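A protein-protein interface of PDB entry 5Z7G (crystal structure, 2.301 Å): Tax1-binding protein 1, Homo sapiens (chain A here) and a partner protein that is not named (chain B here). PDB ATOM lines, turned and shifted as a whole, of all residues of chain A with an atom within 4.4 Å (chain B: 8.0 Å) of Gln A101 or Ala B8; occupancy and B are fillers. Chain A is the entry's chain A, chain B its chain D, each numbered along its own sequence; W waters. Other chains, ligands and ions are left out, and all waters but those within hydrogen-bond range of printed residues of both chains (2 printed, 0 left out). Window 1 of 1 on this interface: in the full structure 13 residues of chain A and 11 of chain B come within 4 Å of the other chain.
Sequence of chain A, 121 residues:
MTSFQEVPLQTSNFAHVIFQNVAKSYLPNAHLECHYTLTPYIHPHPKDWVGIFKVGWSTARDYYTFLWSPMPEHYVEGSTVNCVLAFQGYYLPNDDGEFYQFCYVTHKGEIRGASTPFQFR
Of the 14 printed residues of chain B, 3 touch a printed residue of chain A. Among the printed residues, 5 pairs touch across the chains. Among the printed residues, no Asp or Glu carboxylate lies within 4 Å of a Lys or Arg side-chain nitrogen of the other chain.
Trp A57 touches Ala B8. Ala B8 touches Gln A101 (CB to OE1, 3.5 Å). CB of Ala B8 touches CB of Ala A114, 3.99 Å away. Pro A117 touches Ala B12.
Phe A53 touches none of the printed residues of chain B. Printed residues of chain B within 4 Å of Trp A57: Ser B5 and Ala B8. Gln A101 touches just one residue of chain B: Ala B8. Printed residues of chain B within 4 Å of Ala A114: Ala B8 (3.99 Å). Of the printed residues of chain B, Pro A117 touches Ala B12. Of the printed residues of chain A, Ser B5 touches Trp A57. Of the printed residues of chain A, Ala B8 touches Trp A57, Gln A101 and Ala A114. The nearest residue of chain B that does not touch Gln A101 is Ala B12 (4.3 Å). The nearest printed residue of chain A that does not touch Ser B5 is Gln A101 (6.2 Å).
Water W2 lies within hydrogen-bond range of O of Ser B5 (2.7 Å) and O of Trp A57 (2.8 Å). Water W1 lies within hydrogen-bond range of the side-chain amide oxygen (OE1) of Gln A101, the indole nitrogen (NE1) of Trp A57 and the backbone NH (N) of Leu B9.
The indole nitrogen (NE1) of Trp A57 lies within hydrogen-bond range of the side-chain amide oxygen (OE1) of Gln A101 (2.9 Å). The side-chain amide nitrogen (NE2) of Gln A101 is in hydrogen-bond range of the backbone carbonyl oxygen (O) of Ser A115, 2.9 Å away. SG of Cys A103 is in hydrogen-bond range of NE1 of Trp A57 (3.8 Å). The backbone carbonyl oxygen (O) of Phe A53 lies within hydrogen-bond range of the backbone NH (N) of Gln A101, 2.8 Å away.
O of Trp A57 is in hydrogen-bond range of OG of Ser B5, at 2.9 Å.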
ATOM      1  N   GLY A  51      27.904  19.904 -18.455  1.00  0.00           N
ATOM      2  CA  GLY A  51      27.056  18.769 -18.696  1.00  0.00           C
ATOM      3  C   GLY A  51      26.110  18.594 -17.542  1.00  0.00           C
ATOM      4  O   GLY A  51      26.403  19.024 -16.420  1.00  0.00           O
ATOM      5  N   ILE A  52      24.978  17.955 -17.803  1.00  0.00           N
ATOM      6  CA  ILE A  52      24.065  17.516 -16.762  1.00  0.00           C
ATOM      7  C   ILE A  52      24.288  16.019 -16.592  1.00  0.00           C
ATOM      8  O   ILE A  52      23.965  15.226 -17.481  1.00  0.00           O
ATOM      9  CB  ILE A  52      22.610  17.857 -17.116  1.00  0.00           C
ATOM     10  CG1 ILE A  52      22.395  19.365 -16.966  1.00  0.00           C
ATOM     11  CG2 ILE A  52      21.663  17.110 -16.210  1.00  0.00           C
ATOM     12  CD1 ILE A  52      21.147  19.836 -17.586  1.00  0.00           C
ATOM     13  N   PHE A  53      24.860  15.631 -15.455  1.00  0.00           N
ATOM     14  CA  PHE A  53      25.334  14.272 -15.216  1.00  0.00           C
ATOM     15  C   PHE A  53      24.465  13.585 -14.172  1.00  0.00           C
ATOM     16  O   PHE A  53      24.144  14.171 -13.131  1.00  0.00           O
ATOM     17  CB  PHE A  53      26.790  14.271 -14.718  1.00  0.00           C
ATOM     18  CG  PHE A  53      27.813  14.563 -15.786  1.00  0.00           C
ATOM     19  CD1 PHE A  53      28.082  15.858 -16.171  1.00  0.00           C
ATOM     20  CD2 PHE A  53      28.510  13.535 -16.390  1.00  0.00           C
ATOM     21  CE1 PHE A  53      29.029  16.136 -17.148  1.00  0.00           C
ATOM     22  CE2 PHE A  53      29.445  13.790 -17.381  1.00  0.00           C
ATOM     23  CZ  PHE A  53      29.707  15.100 -17.764  1.00  0.00           C
ATOM     24  N   TRP A  57      28.314   9.329 -11.965  1.00  0.00           N
ATOM     25  CA  TRP A  57      28.969   9.168 -13.252  1.00  0.00           C
ATOM     26  C   TRP A  57      30.436   8.813 -13.063  1.00  0.00           C
ATOM     27  O   TRP A  57      31.063   9.170 -12.060  1.00  0.00           O
ATOM     28  CB  TRP A  57      28.851  10.467 -14.053  1.00  0.00           C
ATOM     29  CG  TRP A  57      29.374  11.660 -13.273  1.00  0.00           C
ATOM     30  CD1 TRP A  57      28.666  12.462 -12.416  1.00  0.00           C
ATOM     31  CD2 TRP A  57      30.719  12.159 -13.261  1.00  0.00           C
ATOM     32  NE1 TRP A  57      29.481  13.437 -11.895  1.00  0.00           N
ATOM     33  CE2 TRP A  57      30.747  13.267 -12.394  1.00  0.00           C
ATOM     34  CE3 TRP A  57      31.901  11.779 -13.909  1.00  0.00           C
ATOM     35  CZ2 TRP A  57      31.913  13.991 -12.149  1.00  0.00           C
ATOM     36  CZ3 TRP A  57      33.050  12.503 -13.665  1.00  0.00           C
ATOM     37  CH2 TRP A  57      33.049  13.592 -12.795  1.00  0.00           C
ATOM     38  N   TYR A 100      20.701  14.355 -10.510  1.00  0.00           N
ATOM     39  CA  TYR A 100      21.597  14.863 -11.522  1.00  0.00           C
ATOM     40  C   TYR A 100      22.386  16.011 -10.915  1.00  0.00           C
ATOM     41  O   TYR A 100      21.987  16.568  -9.894  1.00  0.00           O
ATOM     42  CB  TYR A 100      20.796  15.337 -12.768  1.00  0.00           C
ATOM     43  CG  TYR A 100      20.143  14.189 -13.537  1.00  0.00           C
ATOM     44  CD1 TYR A 100      18.887  13.716 -13.183  1.00  0.00           C
ATOM     45  CD2 TYR A 100      20.806  13.568 -14.594  1.00  0.00           C
ATOM     46  CE1 TYR A 100      18.295  12.652 -13.871  1.00  0.00           C
ATOM     47  CE2 TYR A 100      20.225  12.493 -15.301  1.00  0.00           C
ATOM     48  CZ  TYR A 100      18.976  12.052 -14.929  1.00  0.00           C
ATOM     49  OH  TYR A 100      18.405  11.013 -15.606  1.00  0.00           O
ATOM     50  N   GLN A 101      23.476  16.401 -11.583  1.00  0.00           N
ATOM     51  CA  GLN A 101      24.235  17.573 -11.171  1.00  0.00           C
ATOM     52  C   GLN A 101      24.845  18.227 -12.408  1.00  0.00           C
ATOM     53  O   GLN A 101      24.974  17.596 -13.463  1.00  0.00           O
ATOM     54  CB  GLN A 101      25.313  17.203 -10.129  1.00  0.00           C
ATOM     55  CG  GLN A 101      26.428  16.326 -10.673  1.00  0.00           C
ATOM     56  CD  GLN A 101      27.395  15.809  -9.596  1.00  0.00           C
ATOM     57  OE1 GLN A 101      28.066  14.794  -9.794  1.00  0.00           O
ATOM     58  NE2 GLN A 101      27.474  16.508  -8.465  1.00  0.00           N
ATOM     59  N   PHE A 102      25.170  19.525 -12.289  1.00  0.00           N
ATOM     60  CA  PHE A 102      25.950  20.208 -13.319  1.00  0.00           C
ATOM     61  C   PHE A 102      27.418  19.894 -13.071  1.00  0.00           C
ATOM     62  O   PHE A 102      27.854  19.818 -11.922  1.00  0.00           O
ATOM     63  CB  PHE A 102      25.752  21.738 -13.297  1.00  0.00           C
ATOM     64  CG  PHE A 102      24.311  22.202 -13.530  1.00  0.00           C
ATOM     65  CD1 PHE A 102      23.697  22.047 -14.773  1.00  0.00           C
ATOM     66  CD2 PHE A 102      23.584  22.804 -12.494  1.00  0.00           C
ATOM     67  CE1 PHE A 102      22.382  22.470 -14.997  1.00  0.00           C
ATOM     68  CE2 PHE A 102      22.282  23.246 -12.698  1.00  0.00           C
ATOM     69  CZ  PHE A 102      21.659  23.063 -13.964  1.00  0.00           C
ATOM     70  N   CYS A 103      28.180  19.717 -14.147  1.00  0.00           N
ATOM     71  CA  CYS A 103      29.629  19.586 -14.069  1.00  0.00           C
ATOM     72  C   CYS A 103      30.250  20.434 -15.161  1.00  0.00           C
ATOM     73  O   CYS A 103      29.796  20.391 -16.313  1.00  0.00           O
ATOM     74  CB  CYS A 103      30.080  18.137 -14.253  1.00  0.00           C
ATOM     75  SG  CYS A 103      29.580  17.056 -12.909  1.00  0.00           S
ATOM     76  N   ALA A 114      31.401  20.984  -9.871  1.00  0.00           N
ATOM     77  CA  ALA A 114      30.280  20.064  -9.829  1.00  0.00           C
ATOM     78  C   ALA A 114      29.288  20.538  -8.771  1.00  0.00           C
ATOM     79  O   ALA A 114      29.666  20.731  -7.619  1.00  0.00           O
ATOM     80  CB  ALA A 114      30.769  18.653  -9.522  1.00  0.00           C
ATOM     81  N   SER A 115      28.022  20.702  -9.154  1.00  0.00           N
ATOM     82  CA  SER A 115      27.021  21.305  -8.287  1.00  0.00           C
ATOM     83  C   SER A 115      26.459  20.308  -7.285  1.00  0.00           C
ATOM     84  O   SER A 115      26.653  19.096  -7.392  1.00  0.00           O
ATOM     85  CB  SER A 115      25.857  21.825  -9.120  1.00  0.00           C
ATOM     86  OG  SER A 115      25.107  20.722  -9.619  1.00  0.00           O
ATOM     87  N   THR A 116      25.665  20.833  -6.344  1.00  0.00           N
ATOM     88  CA  THR A 116      24.794  19.974  -5.558  1.00  0.00           C
ATOM     89  C   THR A 116      23.789  19.272  -6.482  1.00  0.00           C
ATOM     90  O   THR A 116      23.496  19.755  -7.576  1.00  0.00           O
ATOM     91  CB  THR A 116      24.061  20.790  -4.502  1.00  0.00           C
ATOM     92  OG1 THR A 116      23.335  21.817  -5.153  1.00  0.00           O
ATOM     93  CG2 THR A 116      25.044  21.452  -3.510  1.00  0.00           C
ATOM     94  N   PRO A 117      23.231  18.140  -6.060  1.00  0.00           N
ATOM     95  CA  PRO A 117      22.376  17.355  -6.952  1.00  0.00           C
ATOM     96  C   PRO A 117      20.918  17.795  -6.928  1.00  0.00           C
ATOM     97  O   PRO A 117      20.437  18.442  -6.001  1.00  0.00           O
ATOM     98  CB  PRO A 117      22.517  15.935  -6.389  1.00  0.00           C
ATOM     99  CG  PRO A 117      22.583  16.172  -4.937  1.00  0.00           C
ATOM    100  CD  PRO A 117      23.417  17.457  -4.772  1.00  0.00           C
ATOM    101  N   PHE A 118      20.209  17.433  -7.991  1.00  0.00           N
ATOM    102  CA  PHE A 118      18.819  17.814  -8.106  1.00  0.00           C
ATOM    103  C   PHE A 118      18.086  16.705  -8.835  1.00  0.00           C
ATOM    104  O   PHE A 118      18.680  15.907  -9.565  1.00  0.00           O
ATOM    105  CB  PHE A 118      18.625  19.147  -8.851  1.00  0.00           C
ATOM    106  CG  PHE A 118      19.546  19.330 -10.022  1.00  0.00           C
ATOM    107  CD1 PHE A 118      19.210  18.807 -11.272  1.00  0.00           C
ATOM    108  CD2 PHE A 118      20.763  19.997  -9.871  1.00  0.00           C
ATOM    109  CE1 PHE A 118      20.051  18.962 -12.362  1.00  0.00           C
ATOM    110  CE2 PHE A 118      21.627  20.149 -10.963  1.00  0.00           C
ATOM    111  CZ  PHE A 118      21.270  19.634 -12.203  1.00  0.00           C
ATOM    112  N   GLU B   1      40.786  12.196 -13.538  1.00  0.00           N
ATOM    113  CA  GLU B   1      39.350  12.166 -13.782  1.00  0.00           C
ATOM    114  C   GLU B   1      38.650  11.166 -12.873  1.00  0.00           C
ATOM    115  O   GLU B   1      37.526  11.397 -12.415  1.00  0.00           O
ATOM    116  CB  GLU B   1      39.043  11.816 -15.239  1.00  0.00           C
ATOM    117  CG  GLU B   1      37.536  11.732 -15.514  1.00  0.00           C
ATOM    118  CD  GLU B   1      37.201  11.196 -16.896  1.00  0.00           C
ATOM    119  OE1 GLU B   1      37.657  10.077 -17.226  1.00  0.00           O
ATOM    120  OE2 GLU B   1      36.479  11.898 -17.645  1.00  0.00           O
ATOM    121  N   SER B   2      39.312  10.033 -12.636  1.00  0.00           N
ATOM    122  CA  SER B   2      38.784   9.075 -11.674  1.00  0.00           C
ATOM    123  C   SER B   2      38.636   9.707 -10.291  1.00  0.00           C
ATOM    124  O   SER B   2      37.678   9.405  -9.567  1.00  0.00           O
ATOM    125  CB  SER B   2      39.693   7.844 -11.626  1.00  0.00           C
ATOM    126  OG  SER B   2      39.375   7.002 -10.534  1.00  0.00           O
ATOM    127  N   VAL B   3      39.559  10.602  -9.919  1.00  0.00           N
ATOM    128  CA  VAL B   3      39.460  11.309  -8.646  1.00  0.00           C
ATOM    129  C   VAL B   3      38.306  12.302  -8.673  1.00  0.00           C
ATOM    130  O   VAL B   3      37.530  12.399  -7.716  1.00  0.00           O
ATOM    131  CB  VAL B   3      40.793  12.008  -8.322  1.00  0.00           C
ATOM    132  CG1 VAL B   3      40.671  12.830  -7.048  1.00  0.00           C
ATOM    133  CG2 VAL B   3      41.915  10.985  -8.214  1.00  0.00           C
ATOM    134  N   ALA B   4      38.173  13.055  -9.763  1.00  0.00           N
ATOM    135  CA  ALA B   4      37.064  13.997  -9.868  1.00  0.00           C
ATOM    136  C   ALA B   4      35.722  13.281  -9.755  1.00  0.00           C
ATOM    137  O   ALA B   4      34.791  13.794  -9.127  1.00  0.00           O
ATOM    138  CB  ALA B   4      37.153  14.775 -11.177  1.00  0.00           C
ATOM    139  N   SER B   5      35.620  12.079 -10.320  1.00  0.00           N
ATOM    140  CA  SER B   5      34.358  11.350 -10.248  1.00  0.00           C
ATOM    141  C   SER B   5      34.030  10.976  -8.814  1.00  0.00           C
ATOM    142  O   SER B   5      32.866  11.055  -8.392  1.00  0.00           O
ATOM    143  CB  SER B   5      34.420  10.102 -11.125  1.00  0.00           C
ATOM    144  OG  SER B   5      33.584   9.086 -10.593  1.00  0.00           O
ATOM    145  N   HIS B   6      35.045  10.582  -8.041  1.00  0.00           N
ATOM    146  CA  HIS B   6      34.817  10.225  -6.643  1.00  0.00           C
ATOM    147  C   HIS B   6      34.479  11.453  -5.800  1.00  0.00           C
ATOM    148  O   HIS B   6      33.583  11.404  -4.946  1.00  0.00           O
ATOM    149  CB  HIS B   6      36.039   9.516  -6.092  1.00  0.00           C
ATOM    150  CG  HIS B   6      35.827   8.919  -4.737  1.00  0.00           C
ATOM    151  ND1 HIS B   6      36.052   9.621  -3.571  1.00  0.00           N
ATOM    152  CD2 HIS B   6      35.434   7.678  -4.363  1.00  0.00           C
ATOM    153  CE1 HIS B   6      35.804   8.838  -2.537  1.00  0.00           C
ATOM    154  NE2 HIS B   6      35.429   7.655  -2.990  1.00  0.00           N
ATOM    155  N   PHE B   7      35.162  12.571  -6.054  1.00  0.00           N
ATOM    156  CA  PHE B   7      34.844  13.811  -5.353  1.00  0.00           C
ATOM    157  C   PHE B   7      33.415  14.263  -5.639  1.00  0.00           C
ATOM    158  O   PHE B   7      32.679  14.634  -4.718  1.00  0.00           O
ATOM    159  CB  PHE B   7      35.841  14.903  -5.743  1.00  0.00           C
ATOM    160  CG  PHE B   7      35.519  16.252  -5.162  1.00  0.00           C
ATOM    161  CD1 PHE B   7      34.851  17.212  -5.920  1.00  0.00           C
ATOM    162  CD2 PHE B   7      35.885  16.568  -3.859  1.00  0.00           C
ATOM    163  CE1 PHE B   7      34.550  18.467  -5.384  1.00  0.00           C
ATOM    164  CE2 PHE B   7      35.589  17.819  -3.317  1.00  0.00           C
ATOM    165  CZ  PHE B   7      34.921  18.769  -4.079  1.00  0.00           C
ATOM    166  N   ALA B   8      33.010  14.264  -6.914  1.00  0.00           N
ATOM    167  CA  ALA B   8      31.670  14.741  -7.236  1.00  0.00           C
ATOM    168  C   ALA B   8      30.611  13.873  -6.582  1.00  0.00           C
ATOM    169  O   ALA B   8      29.543  14.371  -6.216  1.00  0.00           O
ATOM    170  CB  ALA B   8      31.446  14.795  -8.754  1.00  0.00           C
ATOM    171  N   LEU B   9      30.896  12.583  -6.411  1.00  0.00           N
ATOM    172  CA  LEU B   9      29.920  11.692  -5.800  1.00  0.00           C
ATOM    173  C   LEU B   9      29.846  11.906  -4.295  1.00  0.00           C
ATOM    174  O   LEU B   9      28.750  11.894  -3.725  1.00  0.00           O
ATOM    175  CB  LEU B   9      30.265  10.241  -6.136  1.00  0.00           C
ATOM    176  CG  LEU B   9      29.458   9.121  -5.506  1.00  0.00           C
ATOM    177  CD1 LEU B   9      27.970   9.270  -5.822  1.00  0.00           C
ATOM    178  CD2 LEU B   9      29.980   7.772  -6.010  1.00  0.00           C
ATOM    179  N   VAL B  10      30.995  12.128  -3.631  1.00  0.00           N
ATOM    180  CA  VAL B  10      30.962  12.479  -2.207  1.00  0.00           C
ATOM    181  C   VAL B  10      30.172  13.771  -1.985  1.00  0.00           C
ATOM    182  O   VAL B  10      29.329  13.859  -1.086  1.00  0.00           O
ATOM    183  CB  VAL B  10      32.388  12.591  -1.645  1.00  0.00           C
ATOM    184  CG1 VAL B  10      32.338  13.007  -0.179  1.00  0.00           C
ATOM    185  CG2 VAL B  10      33.120  11.272  -1.800  1.00  0.00           C
ATOM    186  N   THR B  11      30.404  14.775  -2.824  1.00  0.00           N
ATOM    187  CA  THR B  11      29.656  16.025  -2.723  1.00  0.00           C
ATOM    188  C   THR B  11      28.154  15.812  -2.887  1.00  0.00           C
ATOM    189  O   THR B  11      27.346  16.409  -2.160  1.00  0.00           O
ATOM    190  CB  THR B  11      30.186  17.000  -3.772  1.00  0.00           C
ATOM    191  OG1 THR B  11      31.518  17.385  -3.409  1.00  0.00           O
ATOM    192  CG2 THR B  11      29.275  18.221  -3.931  1.00  0.00           C
ATOM    193  N   ALA B  12      27.750  14.983  -3.847  1.00  0.00           N
ATOM    194  CA  ALA B  12      26.323  14.722  -3.977  1.00  0.00           C
ATOM    195  C   ALA B  12      25.808  13.939  -2.777  1.00  0.00           C
ATOM    196  O   ALA B  12      24.743  14.254  -2.240  1.00  0.00           O
ATOM    197  CB  ALA B  12      26.040  13.986  -5.284  1.00  0.00           C
ATOM    198  N   TYR B  13      26.563  12.935  -2.324  1.00  0.00           N
ATOM    199  CA  TYR B  13      26.127  12.156  -1.171  1.00  0.00           C
ATOM    200  C   TYR B  13      25.929  13.040   0.061  1.00  0.00           C
ATOM    201  O   TYR B  13      24.922  12.917   0.763  1.00  0.00           O
ATOM    202  CB  TYR B  13      27.135  11.035  -0.887  1.00  0.00           C
ATOM    203  CG  TYR B  13      27.162  10.576   0.563  1.00  0.00           C
ATOM    204  CD1 TYR B  13      26.232   9.652   1.041  1.00  0.00           C
ATOM    205  CD2 TYR B  13      28.114  11.060   1.449  1.00  0.00           C
ATOM    206  CE1 TYR B  13      26.248   9.226   2.373  1.00  0.00           C
ATOM    207  CE2 TYR B  13      28.135  10.645   2.782  1.00  0.00           C
ATOM    208  CZ  TYR B  13      27.192   9.734   3.228  1.00  0.00           C
ATOM    209  OH  TYR B  13      27.212   9.327   4.536  1.00  0.00           O
ATOM    210  N   GLU B  14      26.878  13.942   0.338  1.00  0.00           N
ATOM    211  CA  GLU B  14      26.769  14.799   1.517  1.00  0.00           C
ATOM    212  C   GLU B  14      25.522  15.680   1.469  1.00  0.00           C
ATOM    213  O   GLU B  14      24.892  15.929   2.506  1.00  0.00           O
ATOM    214  CB  GLU B  14      28.018  15.669   1.655  1.00  0.00           C
ATOM    215  CG  GLU B  14      29.316  14.887   1.765  1.00  0.00           C
ATOM    216  CD  GLU B  14      29.543  14.312   3.148  1.00  0.00           C
ATOM    217  OE1 GLU B  14      28.866  14.767   4.100  1.00  0.00           O
ATOM    218  OE2 GLU B  14      30.407  13.415   3.286  1.00  0.00           O
HETATM  219  O   HOH W   1      28.476  12.259  -8.855  1.00  0.00           O
HETATM  220  O   HOH W   2      30.527  10.577  -9.651  1.00  0.00           O
